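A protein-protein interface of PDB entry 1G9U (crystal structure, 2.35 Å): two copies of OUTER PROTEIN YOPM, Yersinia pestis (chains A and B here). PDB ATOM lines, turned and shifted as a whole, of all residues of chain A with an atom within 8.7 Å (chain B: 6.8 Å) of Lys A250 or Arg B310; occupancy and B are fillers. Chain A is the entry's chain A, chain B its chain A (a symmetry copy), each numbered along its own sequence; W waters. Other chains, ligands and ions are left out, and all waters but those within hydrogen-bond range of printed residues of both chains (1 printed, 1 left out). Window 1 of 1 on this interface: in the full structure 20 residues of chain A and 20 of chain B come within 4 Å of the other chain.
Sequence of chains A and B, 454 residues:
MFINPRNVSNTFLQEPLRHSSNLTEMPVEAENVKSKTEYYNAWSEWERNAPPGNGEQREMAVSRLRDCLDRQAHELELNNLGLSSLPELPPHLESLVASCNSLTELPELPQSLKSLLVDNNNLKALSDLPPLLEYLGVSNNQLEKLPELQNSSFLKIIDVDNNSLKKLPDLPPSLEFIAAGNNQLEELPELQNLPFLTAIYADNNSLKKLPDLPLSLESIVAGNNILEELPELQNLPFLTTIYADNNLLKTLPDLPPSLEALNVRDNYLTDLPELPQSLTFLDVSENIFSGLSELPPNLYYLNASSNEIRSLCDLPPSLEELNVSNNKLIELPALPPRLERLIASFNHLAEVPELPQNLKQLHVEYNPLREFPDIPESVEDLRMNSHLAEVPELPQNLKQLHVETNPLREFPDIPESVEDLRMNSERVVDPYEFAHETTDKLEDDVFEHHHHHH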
ATOM      1  N   LYS A 208      19.576  -0.418  24.495  1.00  0.00           N
ATOM      2  CA  LYS A 208      18.377  -0.308  23.658  1.00  0.00           C
ATOM      3  C   LYS A 208      18.662   0.713  22.575  1.00  0.00           C
ATOM      4  O   LYS A 208      17.971   0.757  21.572  1.00  0.00           O
ATOM      5  CB  LYS A 208      17.172   0.142  24.476  1.00  0.00           C
ATOM      6  CG  LYS A 208      17.144  -0.463  25.862  1.00  0.00           C
ATOM      7  CD  LYS A 208      15.776  -0.303  26.503  1.00  0.00           C
ATOM      8  CE  LYS A 208      15.865  -0.795  27.943  1.00  0.00           C
ATOM      9  NZ  LYS A 208      15.065  -2.039  28.163  1.00  0.00           N
ATOM     10  N   ILE A 226      19.824  -4.624  22.529  1.00  0.00           N
ATOM     11  CA  ILE A 226      18.390  -4.756  22.143  1.00  0.00           C
ATOM     12  C   ILE A 226      18.130  -3.554  21.273  1.00  0.00           C
ATOM     13  O   ILE A 226      17.328  -2.674  21.477  1.00  0.00           O
ATOM     14  CB  ILE A 226      17.487  -4.854  23.365  1.00  0.00           C
ATOM     15  CG1 ILE A 226      18.033  -4.172  24.615  1.00  0.00           C
ATOM     16  CG2 ILE A 226      17.187  -6.320  23.674  1.00  0.00           C
ATOM     17  CD1 ILE A 226      17.462  -4.719  25.906  1.00  0.00           C
ATOM     18  N   LEU A 227      18.988  -3.441  20.249  1.00  0.00           N
ATOM     19  CA  LEU A 227      18.884  -2.165  19.532  1.00  0.00           C
ATOM     20  C   LEU A 227      17.637  -2.167  18.685  1.00  0.00           C
ATOM     21  O   LEU A 227      17.310  -3.083  17.922  1.00  0.00           O
ATOM     22  CB  LEU A 227      20.158  -1.921  18.758  1.00  0.00           C
ATOM     23  CG  LEU A 227      21.401  -1.766  19.650  1.00  0.00           C
ATOM     24  CD1 LEU A 227      22.679  -1.853  18.836  1.00  0.00           C
ATOM     25  CD2 LEU A 227      21.302  -0.439  20.421  1.00  0.00           C
ATOM     26  N   GLU A 228      16.897  -1.087  18.936  1.00  0.00           N
ATOM     27  CA  GLU A 228      15.671  -1.000  18.132  1.00  0.00           C
ATOM     28  C   GLU A 228      16.039  -0.162  16.939  1.00  0.00           C
ATOM     29  O   GLU A 228      15.555  -0.156  15.823  1.00  0.00           O
ATOM     30  CB  GLU A 228      14.496  -0.569  18.995  1.00  0.00           C
ATOM     31  CG  GLU A 228      13.220  -1.250  18.485  1.00  0.00           C
ATOM     32  CD  GLU A 228      12.305  -1.791  19.557  1.00  0.00           C
ATOM     33  OE1 GLU A 228      11.079  -1.524  19.511  1.00  0.00           O
ATOM     34  OE2 GLU A 228      12.866  -2.500  20.425  1.00  0.00           O
ATOM     35  N   GLU A 229      17.134   0.594  17.096  1.00  0.00           N
ATOM     36  CA  GLU A 229      17.579   1.269  15.884  1.00  0.00           C
ATOM     37  C   GLU A 229      19.049   1.636  16.123  1.00  0.00           C
ATOM     38  O   GLU A 229      19.470   1.606  17.275  1.00  0.00           O
ATOM     39  CB  GLU A 229      16.759   2.513  15.555  1.00  0.00           C
ATOM     40  CG  GLU A 229      17.233   3.696  16.386  1.00  0.00           C
ATOM     41  CD  GLU A 229      16.308   4.897  16.266  1.00  0.00           C
ATOM     42  OE1 GLU A 229      16.679   5.984  16.777  1.00  0.00           O
ATOM     43  OE2 GLU A 229      15.230   4.718  15.648  1.00  0.00           O
ATOM     44  N   LEU A 230      19.675   1.939  15.003  1.00  0.00           N
ATOM     45  CA  LEU A 230      21.025   2.430  14.906  1.00  0.00           C
ATOM     46  C   LEU A 230      21.016   3.958  14.816  1.00  0.00           C
ATOM     47  O   LEU A 230      20.146   4.529  14.157  1.00  0.00           O
ATOM     48  CB  LEU A 230      21.720   1.895  13.635  1.00  0.00           C
ATOM     49  CG  LEU A 230      21.803   0.366  13.590  1.00  0.00           C
ATOM     50  CD1 LEU A 230      22.529  -0.184  12.376  1.00  0.00           C
ATOM     51  CD2 LEU A 230      22.484  -0.043  14.899  1.00  0.00           C
ATOM     52  N   ASN A 247      19.833  -8.142  17.072  1.00  0.00           N
ATOM     53  CA  ASN A 247      19.200  -7.038  17.781  1.00  0.00           C
ATOM     54  C   ASN A 247      17.743  -6.935  17.360  1.00  0.00           C
ATOM     55  O   ASN A 247      17.054  -7.925  17.084  1.00  0.00           O
ATOM     56  CB  ASN A 247      19.946  -5.739  17.485  1.00  0.00           C
ATOM     57  CG  ASN A 247      21.211  -5.535  18.299  1.00  0.00           C
ATOM     58  OD1 ASN A 247      21.140  -5.252  19.501  1.00  0.00           O
ATOM     59  ND2 ASN A 247      22.350  -5.690  17.617  1.00  0.00           N
ATOM     60  N   LEU A 248      17.174  -5.725  17.346  1.00  0.00           N
ATOM     61  CA  LEU A 248      15.787  -5.731  16.908  1.00  0.00           C
ATOM     62  C   LEU A 248      15.623  -4.818  15.712  1.00  0.00           C
ATOM     63  O   LEU A 248      14.719  -3.992  15.738  1.00  0.00           O
ATOM     64  CB  LEU A 248      14.873  -5.298  18.053  1.00  0.00           C
ATOM     65  CG  LEU A 248      14.865  -6.294  19.222  1.00  0.00           C
ATOM     66  CD1 LEU A 248      14.396  -5.534  20.459  1.00  0.00           C
ATOM     67  CD2 LEU A 248      13.939  -7.466  18.911  1.00  0.00           C
ATOM     68  N   LEU A 249      16.414  -4.917  14.653  1.00  0.00           N
ATOM     69  CA  LEU A 249      16.270  -3.911  13.601  1.00  0.00           C
ATOM     70  C   LEU A 249      15.269  -4.308  12.537  1.00  0.00           C
ATOM     71  O   LEU A 249      15.227  -5.441  12.078  1.00  0.00           O
ATOM     72  CB  LEU A 249      17.654  -3.664  12.984  1.00  0.00           C
ATOM     73  CG  LEU A 249      18.724  -3.244  14.007  1.00  0.00           C
ATOM     74  CD1 LEU A 249      20.102  -3.328  13.369  1.00  0.00           C
ATOM     75  CD2 LEU A 249      18.438  -1.847  14.534  1.00  0.00           C
ATOM     76  N   LYS A 250      14.426  -3.366  12.153  1.00  0.00           N
ATOM     77  CA  LYS A 250      13.412  -3.568  11.118  1.00  0.00           C
ATOM     78  C   LYS A 250      13.849  -2.966   9.787  1.00  0.00           C
ATOM     79  O   LYS A 250      13.417  -3.255   8.670  1.00  0.00           O
ATOM     80  CB  LYS A 250      12.107  -2.901  11.595  1.00  0.00           C
ATOM     81  CG  LYS A 250      11.247  -3.884  12.371  1.00  0.00           C
ATOM     82  CD  LYS A 250      10.364  -3.288  13.440  1.00  0.00           C
ATOM     83  CE  LYS A 250      11.096  -2.672  14.610  1.00  0.00           C
ATOM     84  NZ  LYS A 250      11.387  -3.566  15.760  1.00  0.00           N
ATOM     85  N   THR A 251      14.809  -2.079   9.978  1.00  0.00           N
ATOM     86  CA  THR A 251      15.344  -1.115   9.042  1.00  0.00           C
ATOM     87  C   THR A 251      16.710  -0.615   9.433  1.00  0.00           C
ATOM     88  O   THR A 251      17.033  -0.597  10.630  1.00  0.00           O
ATOM     89  CB  THR A 251      14.354   0.089   9.164  1.00  0.00           C
ATOM     90  OG1 THR A 251      13.820   0.408   7.900  1.00  0.00           O
ATOM     91  CG2 THR A 251      15.065   1.282   9.749  1.00  0.00           C
ATOM     92  N   LEU A 252      17.497  -0.173   8.467  1.00  0.00           N
ATOM     93  CA  LEU A 252      18.825   0.361   8.723  1.00  0.00           C
ATOM     94  C   LEU A 252      18.925   1.814   8.282  1.00  0.00           C
ATOM     95  O   LEU A 252      18.312   2.115   7.254  1.00  0.00           O
ATOM     96  CB  LEU A 252      19.952  -0.352   7.958  1.00  0.00           C
ATOM     97  CG  LEU A 252      20.155  -1.838   8.290  1.00  0.00           C
ATOM     98  CD1 LEU A 252      21.324  -2.374   7.465  1.00  0.00           C
ATOM     99  CD2 LEU A 252      20.368  -2.015   9.792  1.00  0.00           C
ATOM    100  N   PRO A 253      19.771   2.589   8.941  1.00  0.00           N
ATOM    101  CA  PRO A 253      19.940   3.972   8.448  1.00  0.00           C
ATOM    102  C   PRO A 253      20.791   3.922   7.172  1.00  0.00           C
ATOM    103  O   PRO A 253      21.420   2.914   6.806  1.00  0.00           O
ATOM    104  CB  PRO A 253      20.700   4.649   9.579  1.00  0.00           C
ATOM    105  CG  PRO A 253      20.887   3.642  10.672  1.00  0.00           C
ATOM    106  CD  PRO A 253      20.681   2.285  10.052  1.00  0.00           C
ATOM    107  N   ASN A 267      18.175 -10.281  12.264  1.00  0.00           N
ATOM    108  CA  ASN A 267      17.355  -9.115  12.607  1.00  0.00           C
ATOM    109  C   ASN A 267      16.036  -9.310  11.829  1.00  0.00           C
ATOM    110  O   ASN A 267      15.743 -10.461  11.472  1.00  0.00           O
ATOM    111  CB  ASN A 267      18.073  -7.817  12.297  1.00  0.00           C
ATOM    112  CG  ASN A 267      18.995  -7.360  13.409  1.00  0.00           C
ATOM    113  OD1 ASN A 267      18.611  -6.830  14.459  1.00  0.00           O
ATOM    114  ND2 ASN A 267      20.283  -7.558  13.212  1.00  0.00           N
ATOM    115  N   TYR A 268      15.296  -8.232  11.551  1.00  0.00           N
ATOM    116  CA  TYR A 268      13.981  -8.294  10.935  1.00  0.00           C
ATOM    117  C   TYR A 268      13.927  -7.444   9.666  1.00  0.00           C
ATOM    118  O   TYR A 268      12.997  -6.702   9.388  1.00  0.00           O
ATOM    119  CB  TYR A 268      12.874  -7.808  11.856  1.00  0.00           C
ATOM    120  CG  TYR A 268      11.494  -8.437  11.701  1.00  0.00           C
ATOM    121  CD1 TYR A 268      11.241  -9.756  12.067  1.00  0.00           C
ATOM    122  CD2 TYR A 268      10.415  -7.704  11.204  1.00  0.00           C
ATOM    123  CE1 TYR A 268       9.976 -10.325  11.935  1.00  0.00           C
ATOM    124  CE2 TYR A 268       9.136  -8.239  11.054  1.00  0.00           C
ATOM    125  CZ  TYR A 268       8.937  -9.555  11.437  1.00  0.00           C
ATOM    126  OH  TYR A 268       7.696 -10.115  11.300  1.00  0.00           O
ATOM    127  N   LEU A 269      15.017  -7.562   8.936  1.00  0.00           N
ATOM    128  CA  LEU A 269      15.153  -6.758   7.742  1.00  0.00           C
ATOM    129  C   LEU A 269      14.542  -7.437   6.522  1.00  0.00           C
ATOM    130  O   LEU A 269      14.718  -8.618   6.249  1.00  0.00           O
ATOM    131  CB  LEU A 269      16.620  -6.447   7.475  1.00  0.00           C
ATOM    132  CG  LEU A 269      17.357  -5.665   8.564  1.00  0.00           C
ATOM    133  CD1 LEU A 269      18.848  -5.772   8.250  1.00  0.00           C
ATOM    134  CD2 LEU A 269      16.822  -4.241   8.582  1.00  0.00           C
ATOM    135  N   THR A 270      13.835  -6.581   5.809  1.00  0.00           N
ATOM    136  CA  THR A 270      13.196  -6.903   4.554  1.00  0.00           C
ATOM    137  C   THR A 270      13.918  -6.291   3.374  1.00  0.00           C
ATOM    138  O   THR A 270      13.913  -6.798   2.263  1.00  0.00           O
ATOM    139  CB  THR A 270      11.759  -6.340   4.676  1.00  0.00           C
ATOM    140  OG1 THR A 270      10.903  -7.469   4.501  1.00  0.00           O
ATOM    141  CG2 THR A 270      11.520  -5.318   3.617  1.00  0.00           C
ATOM    142  N   ASP A 271      14.548  -5.146   3.616  1.00  0.00           N
ATOM    143  CA  ASP A 271      15.266  -4.415   2.579  1.00  0.00           C
ATOM    144  C   ASP A 271      16.575  -3.851   3.082  1.00  0.00           C
ATOM    145  O   ASP A 271      16.828  -3.747   4.289  1.00  0.00           O
ATOM    146  CB  ASP A 271      14.330  -3.281   2.129  1.00  0.00           C
ATOM    147  CG  ASP A 271      14.773  -2.810   0.757  1.00  0.00           C
ATOM    148  OD1 ASP A 271      14.429  -1.669   0.375  1.00  0.00           O
ATOM    149  OD2 ASP A 271      15.500  -3.548   0.064  1.00  0.00           O
ATOM    150  N   LEU A 272      17.499  -3.432   2.226  1.00  0.00           N
ATOM    151  CA  LEU A 272      18.717  -2.817   2.755  1.00  0.00           C
ATOM    152  C   LEU A 272      18.797  -1.379   2.265  1.00  0.00           C
ATOM    153  O   LEU A 272      18.145  -1.106   1.263  1.00  0.00           O
ATOM    154  CB  LEU A 272      19.988  -3.536   2.309  1.00  0.00           C
ATOM    155  CG  LEU A 272      20.043  -4.920   2.984  1.00  0.00           C
ATOM    156  CD1 LEU A 272      20.850  -5.876   2.144  1.00  0.00           C
ATOM    157  CD2 LEU A 272      20.624  -4.775   4.384  1.00  0.00           C
ATOM    158  N   PRO A 273      19.540  -0.508   2.938  1.00  0.00           N
ATOM    159  CA  PRO A 273      19.724   0.820   2.336  1.00  0.00           C
ATOM    160  C   PRO A 273      20.676   0.619   1.138  1.00  0.00           C
ATOM    161  O   PRO A 273      21.193  -0.485   0.852  1.00  0.00           O
ATOM    162  CB  PRO A 273      20.425   1.589   3.421  1.00  0.00           C
ATOM    163  CG  PRO A 273      20.435   0.747   4.667  1.00  0.00           C
ATOM    164  CD  PRO A 273      20.223  -0.667   4.231  1.00  0.00           C
ATOM    165  N   ASN A 287      17.410 -13.003   8.530  1.00  0.00           N
ATOM    166  CA  ASN A 287      16.589 -11.802   8.383  1.00  0.00           C
ATOM    167  C   ASN A 287      15.336 -12.218   7.666  1.00  0.00           C
ATOM    168  O   ASN A 287      14.868 -13.371   7.697  1.00  0.00           O
ATOM    169  CB  ASN A 287      17.360 -10.718   7.606  1.00  0.00           C
ATOM    170  CG  ASN A 287      18.156  -9.950   8.667  1.00  0.00           C
ATOM    171  OD1 ASN A 287      17.560  -9.080   9.302  1.00  0.00           O
ATOM    172  ND2 ASN A 287      19.410 -10.338   8.890  1.00  0.00           N
ATOM    173  N   ILE A 288      14.678 -11.311   6.946  1.00  0.00           N
ATOM    174  CA  ILE A 288      13.481 -11.887   6.317  1.00  0.00           C
ATOM    175  C   ILE A 288      13.431 -11.488   4.842  1.00  0.00           C
ATOM    176  O   ILE A 288      12.364 -11.071   4.346  1.00  0.00           O
ATOM    177  CB  ILE A 288      12.224 -11.469   7.098  1.00  0.00           C
ATOM    178  CG1 ILE A 288      12.038  -9.951   7.199  1.00  0.00           C
ATOM    179  CG2 ILE A 288      12.177 -12.040   8.510  1.00  0.00           C
ATOM    180  CD1 ILE A 288      10.768  -9.570   7.941  1.00  0.00           C
ATOM    181  N   PHE A 289      14.547 -11.573   4.108  1.00  0.00           N
ATOM    182  CA  PHE A 289      14.615 -11.215   2.699  1.00  0.00           C
ATOM    183  C   PHE A 289      13.974 -12.278   1.799  1.00  0.00           C
ATOM    184  O   PHE A 289      14.266 -13.458   2.067  1.00  0.00           O
ATOM    185  CB  PHE A 289      16.065 -11.110   2.158  1.00  0.00           C
ATOM    186  CG  PHE A 289      16.769  -9.929   2.792  1.00  0.00           C
ATOM    187  CD1 PHE A 289      17.398 -10.100   4.012  1.00  0.00           C
ATOM    188  CD2 PHE A 289      16.760  -8.698   2.153  1.00  0.00           C
ATOM    189  CE1 PHE A 289      18.032  -9.045   4.639  1.00  0.00           C
ATOM    190  CE2 PHE A 289      17.371  -7.644   2.802  1.00  0.00           C
ATOM    191  CZ  PHE A 289      17.974  -7.803   4.029  1.00  0.00           C
ATOM    192  N   PHE B 289       7.331 -14.630  13.378  1.00  0.00           N
ATOM    193  CA  PHE B 289       6.494 -14.147  14.465  1.00  0.00           C
ATOM    194  C   PHE B 289       7.258 -13.219  15.417  1.00  0.00           C
ATOM    195  O   PHE B 289       8.396 -13.604  15.746  1.00  0.00           O
ATOM    196  CB  PHE B 289       5.979 -15.275  15.397  1.00  0.00           C
ATOM    197  CG  PHE B 289       5.002 -16.157  14.648  1.00  0.00           C
ATOM    198  CD1 PHE B 289       5.490 -17.210  13.895  1.00  0.00           C
ATOM    199  CD2 PHE B 289       3.642 -15.891  14.716  1.00  0.00           C
ATOM    200  CE1 PHE B 289       4.637 -18.026  13.177  1.00  0.00           C
ATOM    201  CE2 PHE B 289       2.802 -16.694  13.972  1.00  0.00           C
ATOM    202  CZ  PHE B 289       3.286 -17.724  13.198  1.00  0.00           C
ATOM    203  N   SER B 290       6.580 -12.141  15.826  1.00  0.00           N
ATOM    204  CA  SER B 290       7.257 -11.237  16.763  1.00  0.00           C
ATOM    205  C   SER B 290       6.677 -11.462  18.153  1.00  0.00           C
ATOM    206  O   SER B 290       7.236 -11.001  19.130  1.00  0.00           O
ATOM    207  CB  SER B 290       7.108  -9.760  16.457  1.00  0.00           C
ATOM    208  OG  SER B 290       5.754  -9.542  16.100  1.00  0.00           O
ATOM    209  N   GLY B 291       5.590 -12.203  18.153  1.00  0.00           N
ATOM    210  CA  GLY B 291       4.986 -12.612  19.422  1.00  0.00           C
ATOM    211  C   GLY B 291       4.037 -13.775  19.069  1.00  0.00           C
ATOM    212  O   GLY B 291       3.896 -14.111  17.880  1.00  0.00           O
ATOM    213  N   GLU B 308      11.162 -14.233  15.698  1.00  0.00           N
ATOM    214  CA  GLU B 308      11.739 -12.958  16.149  1.00  0.00           C
ATOM    215  C   GLU B 308      10.959 -12.631  17.418  1.00  0.00           C
ATOM    216  O   GLU B 308      10.504 -11.511  17.592  1.00  0.00           O
ATOM    217  CB  GLU B 308      11.512 -11.850  15.121  1.00  0.00           C
ATOM    218  CG  GLU B 308      12.343 -10.610  15.300  1.00  0.00           C
ATOM    219  CD  GLU B 308      13.839 -10.809  15.298  1.00  0.00           C
ATOM    220  OE1 GLU B 308      14.407 -11.923  15.252  1.00  0.00           O
ATOM    221  OE2 GLU B 308      14.513  -9.758  15.331  1.00  0.00           O
ATOM    222  N   ILE B 309      10.674 -13.638  18.233  1.00  0.00           N
ATOM    223  CA  ILE B 309       9.775 -13.345  19.349  1.00  0.00           C
ATOM    224  C   ILE B 309      10.412 -12.530  20.467  1.00  0.00           C
ATOM    225  O   ILE B 309      11.548 -12.784  20.890  1.00  0.00           O
ATOM    226  CB  ILE B 309       9.245 -14.697  19.846  1.00  0.00           C
ATOM    227  CG1 ILE B 309       8.443 -15.364  18.720  1.00  0.00           C
ATOM    228  CG2 ILE B 309       8.492 -14.582  21.156  1.00  0.00           C
ATOM    229  CD1 ILE B 309       7.909 -16.733  19.190  1.00  0.00           C
ATOM    230  N   ARG B 310       9.639 -11.530  20.880  1.00  0.00           N
ATOM    231  CA  ARG B 310       9.966 -10.513  21.882  1.00  0.00           C
ATOM    232  C   ARG B 310       9.358 -10.819  23.246  1.00  0.00           C
ATOM    233  O   ARG B 310       9.913 -10.570  24.304  1.00  0.00           O
ATOM    234  CB  ARG B 310       9.441  -9.142  21.452  1.00  0.00           C
ATOM    235  CG  ARG B 310      10.001  -8.585  20.135  1.00  0.00           C
ATOM    236  CD  ARG B 310      10.724  -7.283  20.412  1.00  0.00           C
ATOM    237  NE  ARG B 310      10.528  -6.267  19.380  1.00  0.00           N
ATOM    238  CZ  ARG B 310      10.638  -4.978  19.697  1.00  0.00           C
ATOM    239  NH1 ARG B 310      10.922  -4.684  20.953  1.00  0.00           N
ATOM    240  NH2 ARG B 310      10.464  -4.085  18.750  1.00  0.00           N
ATOM    241  N   SER B 311       8.151 -11.407  23.175  1.00  0.00           N
ATOM    242  CA  SER B 311       7.468 -11.653  24.426  1.00  0.00           C
ATOM    243  C   SER B 311       6.520 -12.833  24.196  1.00  0.00           C
ATOM    244  O   SER B 311       6.156 -12.976  23.043  1.00  0.00           O
ATOM    245  CB  SER B 311       6.628 -10.433  24.834  1.00  0.00           C
ATOM    246  OG  SER B 311       5.718 -10.124  23.763  1.00  0.00           O
ATOM    247  N   LEU B 312       6.269 -13.511  25.287  1.00  0.00           N
ATOM    248  CA  LEU B 312       5.382 -14.637  25.488  1.00  0.00           C
ATOM    249  C   LEU B 312       4.374 -14.219  26.530  1.00  0.00           C
ATOM    250  O   LEU B 312       4.640 -13.743  27.625  1.00  0.00           O
ATOM    251  CB  LEU B 312       6.103 -15.927  25.924  1.00  0.00           C
ATOM    252  CG  LEU B 312       6.951 -16.451  24.743  1.00  0.00           C
ATOM    253  CD1 LEU B 312       7.708 -17.728  24.992  1.00  0.00           C
ATOM    254  CD2 LEU B 312       5.988 -16.583  23.572  1.00  0.00           C
ATOM    255  N   ASN B 327      15.387 -16.741  19.896  1.00  0.00           N
ATOM    256  CA  ASN B 327      14.367 -15.713  19.690  1.00  0.00           C
ATOM    257  C   ASN B 327      14.893 -14.396  20.263  1.00  0.00           C
ATOM    258  O   ASN B 327      16.101 -14.250  20.366  1.00  0.00           O
ATOM    259  CB  ASN B 327      12.998 -16.046  20.305  1.00  0.00           C
ATOM    260  CG  ASN B 327      12.208 -16.888  19.319  1.00  0.00           C
ATOM    261  OD1 ASN B 327      11.675 -16.292  18.373  1.00  0.00           O
ATOM    262  ND2 ASN B 327      12.205 -18.214  19.548  1.00  0.00           N
ATOM    263  N   LYS B 328      14.036 -13.453  20.633  1.00  0.00           N
ATOM    264  CA  LYS B 328      14.583 -12.202  21.132  1.00  0.00           C
ATOM    265  C   LYS B 328      14.023 -11.972  22.514  1.00  0.00           C
ATOM    266  O   LYS B 328      13.658 -10.840  22.834  1.00  0.00           O
ATOM    267  CB  LYS B 328      14.170 -11.054  20.203  1.00  0.00           C
ATOM    268  CG  LYS B 328      14.778 -11.249  18.806  1.00  0.00           C
ATOM    269  CD  LYS B 328      16.271 -11.062  18.839  1.00  0.00           C
ATOM    270  CE  LYS B 328      17.087 -11.457  17.639  1.00  0.00           C
ATOM    271  NZ  LYS B 328      16.881 -10.762  16.329  1.00  0.00           N
ATOM    272  N   LEU B 329      13.898 -13.065  23.269  1.00  0.00           N
ATOM    273  CA  LEU B 329      13.281 -12.848  24.579  1.00  0.00           C
ATOM    274  C   LEU B 329      14.251 -12.255  25.604  1.00  0.00           C
ATOM    275  O   LEU B 329      15.426 -12.623  25.547  1.00  0.00           O
ATOM    276  CB  LEU B 329      12.729 -14.179  25.129  1.00  0.00           C
ATOM    277  CG  LEU B 329      11.532 -14.660  24.313  1.00  0.00           C
ATOM    278  CD1 LEU B 329      11.301 -16.137  24.510  1.00  0.00           C
ATOM    279  CD2 LEU B 329      10.278 -13.869  24.660  1.00  0.00           C
ATOM    280  N   ILE B 330      13.721 -11.420  26.505  1.00  0.00           N
ATOM    281  CA  ILE B 330      14.477 -10.937  27.659  1.00  0.00           C
ATOM    282  C   ILE B 330      13.810 -11.432  28.956  1.00  0.00           C
ATOM    283  O   ILE B 330      14.421 -11.439  30.025  1.00  0.00           O
ATOM    284  CB  ILE B 330      14.690  -9.418  27.795  1.00  0.00           C
ATOM    285  CG1 ILE B 330      13.373  -8.654  27.850  1.00  0.00           C
ATOM    286  CG2 ILE B 330      15.599  -8.859  26.704  1.00  0.00           C
ATOM    287  CD1 ILE B 330      13.527  -7.164  28.011  1.00  0.00           C
ATOM    288  N   GLU B 331      12.574 -11.895  28.865  1.00  0.00           N
ATOM    289  CA  GLU B 331      11.913 -12.486  30.031  1.00  0.00           C
ATOM    290  C   GLU B 331      11.079 -13.675  29.575  1.00  0.00           C
ATOM    291  O   GLU B 331      10.523 -13.606  28.470  1.00  0.00           O
ATOM    292  CB  GLU B 331      11.057 -11.412  30.666  1.00  0.00           C
ATOM    293  CG  GLU B 331      10.873 -11.430  32.163  1.00  0.00           C
ATOM    294  CD  GLU B 331       9.833 -10.381  32.562  1.00  0.00           C
ATOM    295  OE1 GLU B 331       9.306 -10.453  33.696  1.00  0.00           O
ATOM    296  OE2 GLU B 331       9.528  -9.498  31.724  1.00  0.00           O
HETATM  297  O   HOH W   1      13.077  -7.051  15.537  1.00  0.00           O
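The side-chain amino group of Lys A250 sits close to the guanidinium group of Arg B310 (3.2 Å).
The side-chain carboxylate (OE1) of Glu A228 is in salt-bridge range of the guanidinium group (NH2) of Arg B310, 2.7 Å away.
NZ of Lys B328 is in hydrogen-bond range of O of Asn A247, at 2.9 Å.
The side-chain amide oxygen (OD1) of Asn A247 is in hydrogen-bond range of the backbone NH (N) of Ile A226 (3.4 Å).
OE2 of Glu B308 is in salt-bridge range of NZ of Lys B328 (2.8 Å).
The backbone NH (N) of Leu A248 lies within hydrogen-bond range of the backbone carbonyl oxygen (O) of Leu A227 (2.7 Å).
The backbone NH (N) of Leu A248 lies within hydrogen-bond range of the side-chain amide oxygen (OD1) of Asn A267.
N of Leu A249 sits at hydrogen-bond distance from OD1 of Asn A267 (2.9 Å).
N of Glu A228 lies within hydrogen-bond range of O of Lys A208, 3.4 Å away.
O of Asn A247 touches OE2 of Glu B308, 3.6 Å away.
Leu A248 touches Arg B310.
Leu A248 touches Lys B328.
C of Asn A267 touches OE2 of Glu B308 (3.8 Å).
CD1 of Tyr A268 touches CG of Glu B308 (3.5 Å).
Of the printed residues of chain B, Glu A228 touches Arg B310.
Printed residues of chain B within 4 Å of Leu A248: Arg B310 and Lys B328.
Printed residues of chain B within 4 Å of Tyr A268: Glu B308 (3.5 Å).
Of the printed residues of chain A, Glu B308 touches Asn A247 (3.6 Å), Asn A267 (3.8 Å) and Tyr A268 (3.5 Å).
Arg B310 touches three residues of chain A.
No residue of chain A comes within 4 Å of Ser B311.
Of the printed residues of chain A, Lys B328 touches Asn A247 and Leu A248.
The nearest printed residue of chain B that does not touch Lys A250 is Glu B308 (6.9 Å).
The nearest residue of chain A that does not touch Arg B310 is Ile A226 (6.7 Å).
Hydrophobic or aromatic side chains of chain A that line the printed part of chain B: Leu A248 and Tyr A268.
Among the printed residues, 8 pairs touch across the chains.
Among the printed residues, Asp or Glu carboxylates within 4 Å of a Lys or Arg side-chain nitrogen of the other chain: Glu A228 with Arg B310 (2.7 Å).
1 position is printed for both chains.
Of the 8 pairs that touch across the chains among the printed residues, none has its exchanged pair printed and touching as well.
Water W1 lies within hydrogen-bond range of the side-chain carboxylate (OE2) of Glu B308 and the backbone carbonyl oxygen (O) of Leu A248.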
